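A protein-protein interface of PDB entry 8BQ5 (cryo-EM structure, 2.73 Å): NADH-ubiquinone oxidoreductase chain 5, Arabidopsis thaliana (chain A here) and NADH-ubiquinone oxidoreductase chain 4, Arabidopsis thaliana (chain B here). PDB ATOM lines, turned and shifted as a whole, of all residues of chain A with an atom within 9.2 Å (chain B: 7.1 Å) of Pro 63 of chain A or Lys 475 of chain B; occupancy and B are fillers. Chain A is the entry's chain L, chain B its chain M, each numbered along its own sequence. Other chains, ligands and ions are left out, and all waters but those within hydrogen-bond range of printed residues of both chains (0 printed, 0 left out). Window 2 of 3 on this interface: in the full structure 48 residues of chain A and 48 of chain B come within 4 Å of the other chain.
Printed residues of chain B within 4 Å of Pro 63 of chain A: Tyr 473 and Lys 475. Of the printed residues of chain B, Trp 64 of chain A touches Val 472 (3.1 Å) and Pro 474 (3.1 Å). Phe 70 of chain A touches none of the printed residues of chain B. Met 470 of chain B touches none of the printed residues of chain A. Of the printed residues of chain A, Val 472 of chain B touches Trp 64 and Trp 74. Of chain A, only Trp 64 comes within 4 Å of Pro 474 of chain B. No residue of chain A comes within 4 Å of Val 476 of chain B. Of the printed residues of chain A, His 482 of chain B touches Ser 66 (3.5 Å) and Ser 67 (3.5 Å). The nearest residue of chain B that does not touch Pro 63 of chain A is Val 472 of chain B (4.6 Å). The nearest residue of chain A that does not touch Lys 475 of chain B is Trp 64 of chain A (4.9 Å).
Among the printed residues, pairs that only touch across the chains: Trp 64 of chain A with Pro 474 of chain B, Trp 64 of chain A with Val 472 of chain B, Ser 66 of chain A with His 482 of chain B, Ser 66 of chain A with Leu 478 of chain B, Pro 63 of chain A with Tyr 473 of chain B and Pro 63 of chain A with Lys 475 of chain B.
Printed residues of chain B that touch a printed residue of chain A: Val 472, Tyr 473, Pro 474, Lys 475, Leu 478 and His 482. Hydrophobic or aromatic side chains of chain B within 4 Å of the printed part of chain A: Tyr 473, Pro 474, Leu 478 and His 482. Printed residues of chain A that touch a printed residue of chain B: Pro 63, Trp 64, Ser 66, Ser 67 and Trp 74. Among the printed residues, 8 pairs touch across the chains.
A ring nitrogen (NE2) of His 482 of chain B lies within hydrogen-bond range of the side-chain hydroxyl (OG) of Ser 67 of chain A, 3.5 Å away. The backbone carbonyl oxygen (O) of Val 472 of chain B is in hydrogen-bond range of the indole nitrogen (NE1) of Trp 74 of chain A, at 3.0 Å.
The backbone NH (N) of Ile 61 of chain A sits at hydrogen-bond distance from the backbone carbonyl oxygen (O) of Trp 74 of chain A. The backbone NH of Trp 74 of chain A lies within hydrogen-bond range of the backbone carbonyl oxygen of Ala 62 of chain A. N of Trp 64 of chain A sits at hydrogen-bond distance from O of Ala 72 of chain A, 3.0 Å away. NZ of Lys 475 of chain B lies within salt-bridge range of OD2 of Asp 479 of chain B, 3.0 Å away. The backbone carbonyl oxygen (O) of Leu 478 of chain B lies within hydrogen-bond range of a ring nitrogen (ND1) of His 482 of chain B (3.1 Å).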
ATOM      1  N   ARG A  60      -3.791   4.433  18.861  1.00  0.00           N
ATOM      2  CA  ARG A  60      -5.096   4.713  19.444  1.00  0.00           C
ATOM      3  C   ARG A  60      -5.743   3.393  19.829  1.00  0.00           C
ATOM      4  O   ARG A  60      -5.851   2.488  18.995  1.00  0.00           O
ATOM      5  CB  ARG A  60      -5.986   5.480  18.469  1.00  0.00           C
ATOM      6  CG  ARG A  60      -7.104   6.244  19.143  1.00  0.00           C
ATOM      7  CD  ARG A  60      -7.819   7.163  18.168  1.00  0.00           C
ATOM      8  NE  ARG A  60      -9.164   7.520  18.611  1.00  0.00           N
ATOM      9  CZ  ARG A  60     -10.140   6.658  18.871  1.00  0.00           C
ATOM     10  NH1 ARG A  60      -9.993   5.358  18.669  1.00  0.00           N
ATOM     11  NH2 ARG A  60     -11.300   7.114  19.331  1.00  0.00           N
ATOM     12  N   ILE A  61      -6.174   3.283  21.083  1.00  0.00           N
ATOM     13  CA  ILE A  61      -6.812   2.053  21.541  1.00  0.00           C
ATOM     14  C   ILE A  61      -8.325   2.146  21.394  1.00  0.00           C
ATOM     15  O   ILE A  61      -8.941   1.389  20.636  1.00  0.00           O
ATOM     16  CB  ILE A  61      -6.410   1.743  22.993  1.00  0.00           C
ATOM     17  CG1 ILE A  61      -4.900   1.533  23.097  1.00  0.00           C
ATOM     18  CG2 ILE A  61      -7.157   0.524  23.501  1.00  0.00           C
ATOM     19  CD1 ILE A  61      -4.450   1.032  24.448  1.00  0.00           C
ATOM     20  N   ALA A  62      -8.937   3.083  22.102  1.00  0.00           N
ATOM     21  CA  ALA A  62     -10.385   3.229  22.123  1.00  0.00           C
ATOM     22  C   ALA A  62     -10.714   4.638  22.593  1.00  0.00           C
ATOM     23  O   ALA A  62      -9.872   5.296  23.209  1.00  0.00           O
ATOM     24  CB  ALA A  62     -11.038   2.187  23.047  1.00  0.00           C
ATOM     25  N   PRO A  63     -11.916   5.128  22.298  1.00  0.00           N
ATOM     26  CA  PRO A  63     -12.345   6.398  22.890  1.00  0.00           C
ATOM     27  C   PRO A  63     -12.478   6.261  24.397  1.00  0.00           C
ATOM     28  O   PRO A  63     -12.829   5.200  24.915  1.00  0.00           O
ATOM     29  CB  PRO A  63     -13.699   6.658  22.223  1.00  0.00           C
ATOM     30  CG  PRO A  63     -14.185   5.292  21.863  1.00  0.00           C
ATOM     31  CD  PRO A  63     -12.950   4.580  21.403  1.00  0.00           C
ATOM     32  N   TRP A  64     -12.183   7.348  25.106  1.00  0.00           N
ATOM     33  CA  TRP A  64     -12.363   7.378  26.552  1.00  0.00           C
ATOM     34  C   TRP A  64     -13.589   8.199  26.938  1.00  0.00           C
ATOM     35  O   TRP A  64     -14.524   7.670  27.541  1.00  0.00           O
ATOM     36  CB  TRP A  64     -11.096   7.924  27.223  1.00  0.00           C
ATOM     37  CG  TRP A  64     -11.158   7.960  28.717  1.00  0.00           C
ATOM     38  CD1 TRP A  64     -11.988   7.238  29.523  1.00  0.00           C
ATOM     39  CD2 TRP A  64     -10.335   8.744  29.586  1.00  0.00           C
ATOM     40  NE1 TRP A  64     -11.743   7.535  30.840  1.00  0.00           N
ATOM     41  CE2 TRP A  64     -10.731   8.456  30.906  1.00  0.00           C
ATOM     42  CE3 TRP A  64      -9.306   9.666  29.376  1.00  0.00           C
ATOM     43  CZ2 TRP A  64     -10.135   9.057  32.011  1.00  0.00           C
ATOM     44  CZ3 TRP A  64      -8.715  10.260  30.474  1.00  0.00           C
ATOM     45  CH2 TRP A  64      -9.131   9.954  31.774  1.00  0.00           C
ATOM     46  N   ILE A  65     -13.622   9.472  26.560  1.00  0.00           N
ATOM     47  CA  ILE A  65     -14.727  10.367  26.891  1.00  0.00           C
ATOM     48  C   ILE A  65     -15.130  11.068  25.602  1.00  0.00           C
ATOM     49  O   ILE A  65     -14.508  12.060  25.206  1.00  0.00           O
ATOM     50  CB  ILE A  65     -14.359  11.383  27.976  1.00  0.00           C
ATOM     51  CG1 ILE A  65     -13.762  10.682  29.196  1.00  0.00           C
ATOM     52  CG2 ILE A  65     -15.580  12.196  28.373  1.00  0.00           C
ATOM     53  CD1 ILE A  65     -12.778  11.530  29.964  1.00  0.00           C
ATOM     54  N   SER A  66     -16.168  10.561  24.945  1.00  0.00           N
ATOM     55  CA  SER A  66     -16.693  11.152  23.718  1.00  0.00           C
ATOM     56  C   SER A  66     -18.072  11.727  24.013  1.00  0.00           C
ATOM     57  O   SER A  66     -19.030  10.979  24.235  1.00  0.00           O
ATOM     58  CB  SER A  66     -16.753  10.120  22.595  1.00  0.00           C
ATOM     59  OG  SER A  66     -16.696  10.751  21.330  1.00  0.00           O
ATOM     60  N   SER A  67     -18.172  13.055  24.004  1.00  0.00           N
ATOM     61  CA  SER A  67     -19.428  13.755  24.268  1.00  0.00           C
ATOM     62  C   SER A  67     -19.447  14.998  23.383  1.00  0.00           C
ATOM     63  O   SER A  67     -18.833  16.013  23.722  1.00  0.00           O
ATOM     64  CB  SER A  67     -19.560  14.114  25.742  1.00  0.00           C
ATOM     65  OG  SER A  67     -20.808  14.728  26.008  1.00  0.00           O
ATOM     66  N   PHE A  70     -16.144  16.933  22.573  1.00  0.00           N
ATOM     67  CA  PHE A  70     -15.136  16.495  23.532  1.00  0.00           C
ATOM     68  C   PHE A  70     -14.669  15.086  23.188  1.00  0.00           C
ATOM     69  O   PHE A  70     -15.464  14.144  23.181  1.00  0.00           O
ATOM     70  CB  PHE A  70     -15.709  16.552  24.947  1.00  0.00           C
ATOM     71  CG  PHE A  70     -14.672  16.468  26.030  1.00  0.00           C
ATOM     72  CD1 PHE A  70     -14.460  15.282  26.711  1.00  0.00           C
ATOM     73  CD2 PHE A  70     -13.912  17.575  26.370  1.00  0.00           C
ATOM     74  CE1 PHE A  70     -13.508  15.200  27.709  1.00  0.00           C
ATOM     75  CE2 PHE A  70     -12.959  17.500  27.365  1.00  0.00           C
ATOM     76  CZ  PHE A  70     -12.757  16.310  28.037  1.00  0.00           C
ATOM     77  N   ASP A  71     -13.370  14.943  22.925  1.00  0.00           N
ATOM     78  CA  ASP A  71     -12.828  13.783  22.226  1.00  0.00           C
ATOM     79  C   ASP A  71     -11.654  13.166  22.973  1.00  0.00           C
ATOM     80  O   ASP A  71     -10.645  12.791  22.369  1.00  0.00           O
ATOM     81  CB  ASP A  71     -12.398  14.171  20.816  1.00  0.00           C
ATOM     82  CG  ASP A  71     -11.355  15.276  20.815  1.00  0.00           C
ATOM     83  OD1 ASP A  71     -11.338  16.075  21.772  1.00  0.00           O
ATOM     84  OD2 ASP A  71     -10.549  15.340  19.864  1.00  0.00           O
ATOM     85  N   ALA A  72     -11.754  13.042  24.291  1.00  0.00           N
ATOM     86  CA  ALA A  72     -10.698  12.373  25.038  1.00  0.00           C
ATOM     87  C   ALA A  72     -10.691  10.885  24.715  1.00  0.00           C
ATOM     88  O   ALA A  72     -11.741  10.241  24.658  1.00  0.00           O
ATOM     89  CB  ALA A  72     -10.883  12.592  26.538  1.00  0.00           C
ATOM     90  N   SER A  73      -9.480  10.387  24.452  1.00  0.00           N
ATOM     91  CA  SER A  73      -9.342   8.969  24.060  1.00  0.00           C
ATOM     92  C   SER A  73      -8.168   8.289  24.752  1.00  0.00           C
ATOM     93  O   SER A  73      -7.391   8.980  25.427  1.00  0.00           O
ATOM     94  CB  SER A  73      -9.158   8.853  22.576  1.00  0.00           C
ATOM     95  OG  SER A  73      -7.940   9.455  22.171  1.00  0.00           O
ATOM     96  N   TRP A  74      -8.114   6.970  24.651  1.00  0.00           N
ATOM     97  CA  TRP A  74      -6.960   6.195  25.100  1.00  0.00           C
ATOM     98  C   TRP A  74      -5.994   6.103  23.928  1.00  0.00           C
ATOM     99  O   TRP A  74      -6.024   5.157  23.141  1.00  0.00           O
ATOM    100  CB  TRP A  74      -7.381   4.814  25.582  1.00  0.00           C
ATOM    101  CG  TRP A  74      -8.289   4.826  26.766  1.00  0.00           C
ATOM    102  CD1 TRP A  74      -9.595   4.442  26.796  1.00  0.00           C
ATOM    103  CD2 TRP A  74      -7.955   5.222  28.101  1.00  0.00           C
ATOM    104  NE1 TRP A  74     -10.101   4.585  28.064  1.00  0.00           N
ATOM    105  CE2 TRP A  74      -9.114   5.061  28.884  1.00  0.00           C
ATOM    106  CE3 TRP A  74      -6.792   5.704  28.708  1.00  0.00           C
ATOM    107  CZ2 TRP A  74      -9.143   5.363  30.243  1.00  0.00           C
ATOM    108  CZ3 TRP A  74      -6.823   6.002  30.056  1.00  0.00           C
ATOM    109  CH2 TRP A  74      -7.991   5.830  30.810  1.00  0.00           C
ATOM    110  N   GLY A  75      -5.141   7.122  23.816  1.00  0.00           N
ATOM    111  CA  GLY A  75      -4.204   7.200  22.681  1.00  0.00           C
ATOM    112  C   GLY A  75      -2.792   7.504  23.122  1.00  0.00           C
ATOM    113  O   GLY A  75      -2.625   8.270  24.083  1.00  0.00           O
ATOM    114  N   ASN A 132      -3.277  13.310  24.349  1.00  0.00           N
ATOM    115  CA  ASN A 132      -4.366  14.289  24.608  1.00  0.00           C
ATOM    116  C   ASN A 132      -4.255  14.807  26.041  1.00  0.00           C
ATOM    117  O   ASN A 132      -3.617  14.139  26.867  1.00  0.00           O
ATOM    118  CB  ASN A 132      -5.747  13.723  24.277  1.00  0.00           C
ATOM    119  CG  ASN A 132      -6.105  12.481  25.061  1.00  0.00           C
ATOM    120  OD1 ASN A 132      -6.669  12.571  26.145  1.00  0.00           O
ATOM    121  ND2 ASN A 132      -5.799  11.319  24.511  1.00  0.00           N
ATOM    122  N   GLN A 135      -5.683  12.169  28.798  1.00  0.00           N
ATOM    123  CA  GLN A 135      -4.789  11.056  29.088  1.00  0.00           C
ATOM    124  C   GLN A 135      -3.571  11.534  29.869  1.00  0.00           C
ATOM    125  O   GLN A 135      -3.068  10.826  30.749  1.00  0.00           O
ATOM    126  CB  GLN A 135      -4.369  10.369  27.790  1.00  0.00           C
ATOM    127  CG  GLN A 135      -3.270   9.345  27.962  1.00  0.00           C
ATOM    128  CD  GLN A 135      -3.563   8.042  27.260  1.00  0.00           C
ATOM    129  OE1 GLN A 135      -4.657   7.835  26.737  1.00  0.00           O
ATOM    130  NE2 GLN A 135      -2.575   7.161  27.222  1.00  0.00           N
ATOM    131  N   LEU B 336     -24.322  11.261  34.517  1.00  0.00           N
ATOM    132  CA  LEU B 336     -23.281  10.285  34.819  1.00  0.00           C
ATOM    133  C   LEU B 336     -22.823  10.390  36.268  1.00  0.00           C
ATOM    134  O   LEU B 336     -22.555   9.373  36.915  1.00  0.00           O
ATOM    135  CB  LEU B 336     -22.106  10.462  33.863  1.00  0.00           C
ATOM    136  CG  LEU B 336     -22.322   9.836  32.484  1.00  0.00           C
ATOM    137  CD1 LEU B 336     -21.006   9.694  31.745  1.00  0.00           C
ATOM    138  CD2 LEU B 336     -23.017   8.487  32.610  1.00  0.00           C
ATOM    139  N   TRP B 469     -15.799   0.273  35.299  1.00  0.00           N
ATOM    140  CA  TRP B 469     -16.384   0.165  33.964  1.00  0.00           C
ATOM    141  C   TRP B 469     -16.788   1.530  33.418  1.00  0.00           C
ATOM    142  O   TRP B 469     -16.397   1.907  32.308  1.00  0.00           O
ATOM    143  CB  TRP B 469     -17.585  -0.778  34.006  1.00  0.00           C
ATOM    144  CG  TRP B 469     -18.239  -1.015  32.684  1.00  0.00           C
ATOM    145  CD1 TRP B 469     -17.702  -0.801  31.448  1.00  0.00           C
ATOM    146  CD2 TRP B 469     -19.560  -1.518  32.465  1.00  0.00           C
ATOM    147  NE1 TRP B 469     -18.608  -1.136  30.474  1.00  0.00           N
ATOM    148  CE2 TRP B 469     -19.758  -1.580  31.073  1.00  0.00           C
ATOM    149  CE3 TRP B 469     -20.597  -1.920  33.313  1.00  0.00           C
ATOM    150  CZ2 TRP B 469     -20.949  -2.028  30.509  1.00  0.00           C
ATOM    151  CZ3 TRP B 469     -21.777  -2.366  32.750  1.00  0.00           C
ATOM    152  CH2 TRP B 469     -21.943  -2.415  31.362  1.00  0.00           C
ATOM    153  N   MET B 470     -17.573   2.288  34.184  1.00  0.00           N
ATOM    154  CA  MET B 470     -17.953   3.623  33.737  1.00  0.00           C
ATOM    155  C   MET B 470     -16.755   4.565  33.748  1.00  0.00           C
ATOM    156  O   MET B 470     -16.720   5.536  32.985  1.00  0.00           O
ATOM    157  CB  MET B 470     -19.089   4.164  34.610  1.00  0.00           C
ATOM    158  CG  MET B 470     -19.471   5.617  34.344  1.00  0.00           C
ATOM    159  SD  MET B 470     -20.863   6.220  35.327  1.00  0.00           S
ATOM    160  CE  MET B 470     -21.768   4.705  35.635  1.00  0.00           C
ATOM    161  N   VAL B 472     -13.532   3.960  32.835  1.00  0.00           N
ATOM    162  CA  VAL B 472     -12.588   3.841  31.727  1.00  0.00           C
ATOM    163  C   VAL B 472     -13.311   3.792  30.384  1.00  0.00           C
ATOM    164  O   VAL B 472     -12.768   4.236  29.367  1.00  0.00           O
ATOM    165  CB  VAL B 472     -11.667   2.616  31.896  1.00  0.00           C
ATOM    166  CG1 VAL B 472     -10.923   2.689  33.220  1.00  0.00           C
ATOM    167  CG2 VAL B 472     -12.448   1.315  31.781  1.00  0.00           C
ATOM    168  N   TYR B 473     -14.529   3.255  30.359  1.00  0.00           N
ATOM    169  CA  TYR B 473     -15.318   3.158  29.128  1.00  0.00           C
ATOM    170  C   TYR B 473     -16.740   3.639  29.378  1.00  0.00           C
ATOM    171  O   TYR B 473     -17.687   2.844  29.414  1.00  0.00           O
ATOM    172  CB  TYR B 473     -15.316   1.727  28.588  1.00  0.00           C
ATOM    173  CG  TYR B 473     -15.647   1.636  27.115  1.00  0.00           C
ATOM    174  CD1 TYR B 473     -14.803   2.182  26.160  1.00  0.00           C
ATOM    175  CD2 TYR B 473     -16.815   1.021  26.683  1.00  0.00           C
ATOM    176  CE1 TYR B 473     -15.103   2.105  24.814  1.00  0.00           C
ATOM    177  CE2 TYR B 473     -17.124   0.940  25.338  1.00  0.00           C
ATOM    178  CZ  TYR B 473     -16.264   1.484  24.409  1.00  0.00           C
ATOM    179  OH  TYR B 473     -16.564   1.408  23.069  1.00  0.00           O
ATOM    180  N   PRO B 474     -16.933   4.951  29.540  1.00  0.00           N
ATOM    181  CA  PRO B 474     -18.291   5.479  29.722  1.00  0.00           C
ATOM    182  C   PRO B 474     -19.099   5.588  28.438  1.00  0.00           C
ATOM    183  O   PRO B 474     -20.151   6.236  28.449  1.00  0.00           O
ATOM    184  CB  PRO B 474     -18.041   6.865  30.328  1.00  0.00           C
ATOM    185  CG  PRO B 474     -16.726   7.263  29.781  1.00  0.00           C
ATOM    186  CD  PRO B 474     -15.913   6.002  29.705  1.00  0.00           C
ATOM    187  N   LYS B 475     -18.653   4.981  27.335  1.00  0.00           N
ATOM    188  CA  LYS B 475     -19.355   5.148  26.066  1.00  0.00           C
ATOM    189  C   LYS B 475     -20.647   4.340  26.026  1.00  0.00           C
ATOM    190  O   LYS B 475     -21.612   4.752  25.373  1.00  0.00           O
ATOM    191  CB  LYS B 475     -18.433   4.766  24.904  1.00  0.00           C
ATOM    192  CG  LYS B 475     -19.082   4.813  23.524  1.00  0.00           C
ATOM    193  CD  LYS B 475     -18.051   4.638  22.414  1.00  0.00           C
ATOM    194  CE  LYS B 475     -18.701   4.223  21.100  1.00  0.00           C
ATOM    195  NZ  LYS B 475     -19.364   2.893  21.201  1.00  0.00           N
ATOM    196  N   VAL B 476     -20.694   3.201  26.723  1.00  0.00           N
ATOM    197  CA  VAL B 476     -21.912   2.395  26.746  1.00  0.00           C
ATOM    198  C   VAL B 476     -23.067   3.185  27.343  1.00  0.00           C
ATOM    199  O   VAL B 476     -24.225   3.022  26.941  1.00  0.00           O
ATOM    200  CB  VAL B 476     -21.679   1.078  27.512  1.00  0.00           C
ATOM    201  CG1 VAL B 476     -21.031   0.050  26.608  1.00  0.00           C
ATOM    202  CG2 VAL B 476     -20.836   1.321  28.754  1.00  0.00           C
ATOM    203  N   PHE B 477     -22.774   4.051  28.313  1.00  0.00           N
ATOM    204  CA  PHE B 477     -23.818   4.866  28.920  1.00  0.00           C
ATOM    205  C   PHE B 477     -24.116   6.102  28.079  1.00  0.00           C
ATOM    206  O   PHE B 477     -25.281   6.417  27.816  1.00  0.00           O
ATOM    207  CB  PHE B 477     -23.410   5.259  30.341  1.00  0.00           C
ATOM    208  CG  PHE B 477     -23.121   4.085  31.232  1.00  0.00           C
ATOM    209  CD1 PHE B 477     -24.147   3.430  31.891  1.00  0.00           C
ATOM    210  CD2 PHE B 477     -21.823   3.632  31.407  1.00  0.00           C
ATOM    211  CE1 PHE B 477     -23.885   2.346  32.708  1.00  0.00           C
ATOM    212  CE2 PHE B 477     -21.556   2.550  32.223  1.00  0.00           C
ATOM    213  CZ  PHE B 477     -22.590   1.906  32.875  1.00  0.00           C
ATOM    214  N   LEU B 478     -23.071   6.805  27.636  1.00  0.00           N
ATOM    215  CA  LEU B 478     -23.263   8.029  26.863  1.00  0.00           C
ATOM    216  C   LEU B 478     -23.926   7.754  25.518  1.00  0.00           C
ATOM    217  O   LEU B 478     -24.621   8.626  24.984  1.00  0.00           O
ATOM    218  CB  LEU B 478     -21.920   8.733  26.671  1.00  0.00           C
ATOM    219  CG  LEU B 478     -21.334   9.426  27.907  1.00  0.00           C
ATOM    220  CD1 LEU B 478     -19.895   9.852  27.664  1.00  0.00           C
ATOM    221  CD2 LEU B 478     -22.177  10.623  28.310  1.00  0.00           C
ATOM    222  N   ASP B 479     -23.725   6.559  24.956  1.00  0.00           N
ATOM    223  CA  ASP B 479     -24.372   6.215  23.694  1.00  0.00           C
ATOM    224  C   ASP B 479     -25.887   6.155  23.839  1.00  0.00           C
ATOM    225  O   ASP B 479     -26.620   6.600  22.949  1.00  0.00           O
ATOM    226  CB  ASP B 479     -23.842   4.880  23.177  1.00  0.00           C
ATOM    227  CG  ASP B 479     -22.579   5.035  22.365  1.00  0.00           C
ATOM    228  OD1 ASP B 479     -22.182   6.190  22.105  1.00  0.00           O
ATOM    229  OD2 ASP B 479     -21.983   4.005  21.990  1.00  0.00           O
ATOM    230  N   CYS B 480     -26.374   5.597  24.947  1.00  0.00           N
ATOM    231  CA  CYS B 480     -27.806   5.432  25.151  1.00  0.00           C
ATOM    232  C   CYS B 480     -28.481   6.681  25.696  1.00  0.00           C
ATOM    233  O   CYS B 480     -29.706   6.682  25.854  1.00  0.00           O
ATOM    234  CB  CYS B 480     -28.070   4.261  26.100  1.00  0.00           C
ATOM    235  SG  CYS B 480     -27.485   2.657  25.501  1.00  0.00           S
ATOM    236  N   MET B 481     -27.726   7.737  25.991  1.00  0.00           N
ATOM    237  CA  MET B 481     -28.294   8.941  26.583  1.00  0.00           C
ATOM    238  C   MET B 481     -28.309  10.137  25.648  1.00  0.00           C
ATOM    239  O   MET B 481     -29.099  11.058  25.864  1.00  0.00           O
ATOM    240  CB  MET B 481     -27.519   9.327  27.848  1.00  0.00           C
ATOM    241  CG  MET B 481     -27.767   8.427  29.046  1.00  0.00           C
ATOM    242  SD  MET B 481     -26.510   8.581  30.330  1.00  0.00           S
ATOM    243  CE  MET B 481     -25.440   9.833  29.627  1.00  0.00           C
ATOM    244  N   HIS B 482     -27.477  10.136  24.606  1.00  0.00           N
ATOM    245  CA  HIS B 482     -27.178  11.374  23.892  1.00  0.00           C
ATOM    246  C   HIS B 482     -28.381  11.914  23.126  1.00  0.00           C
ATOM    247  O   HIS B 482     -28.565  13.132  23.037  1.00  0.00           O
ATOM    248  CB  HIS B 482     -25.994  11.163  22.953  1.00  0.00           C
ATOM    249  CG  HIS B 482     -24.681  11.537  23.563  1.00  0.00           C
ATOM    250  ND1 HIS B 482     -23.501  10.900  23.246  1.00  0.00           N
ATOM    251  CD2 HIS B 482     -24.367  12.474  24.488  1.00  0.00           C
ATOM    252  CE1 HIS B 482     -22.515  11.436  23.942  1.00  0.00           C
ATOM    253  NE2 HIS B 482     -23.013  12.394  24.703  1.00  0.00           N
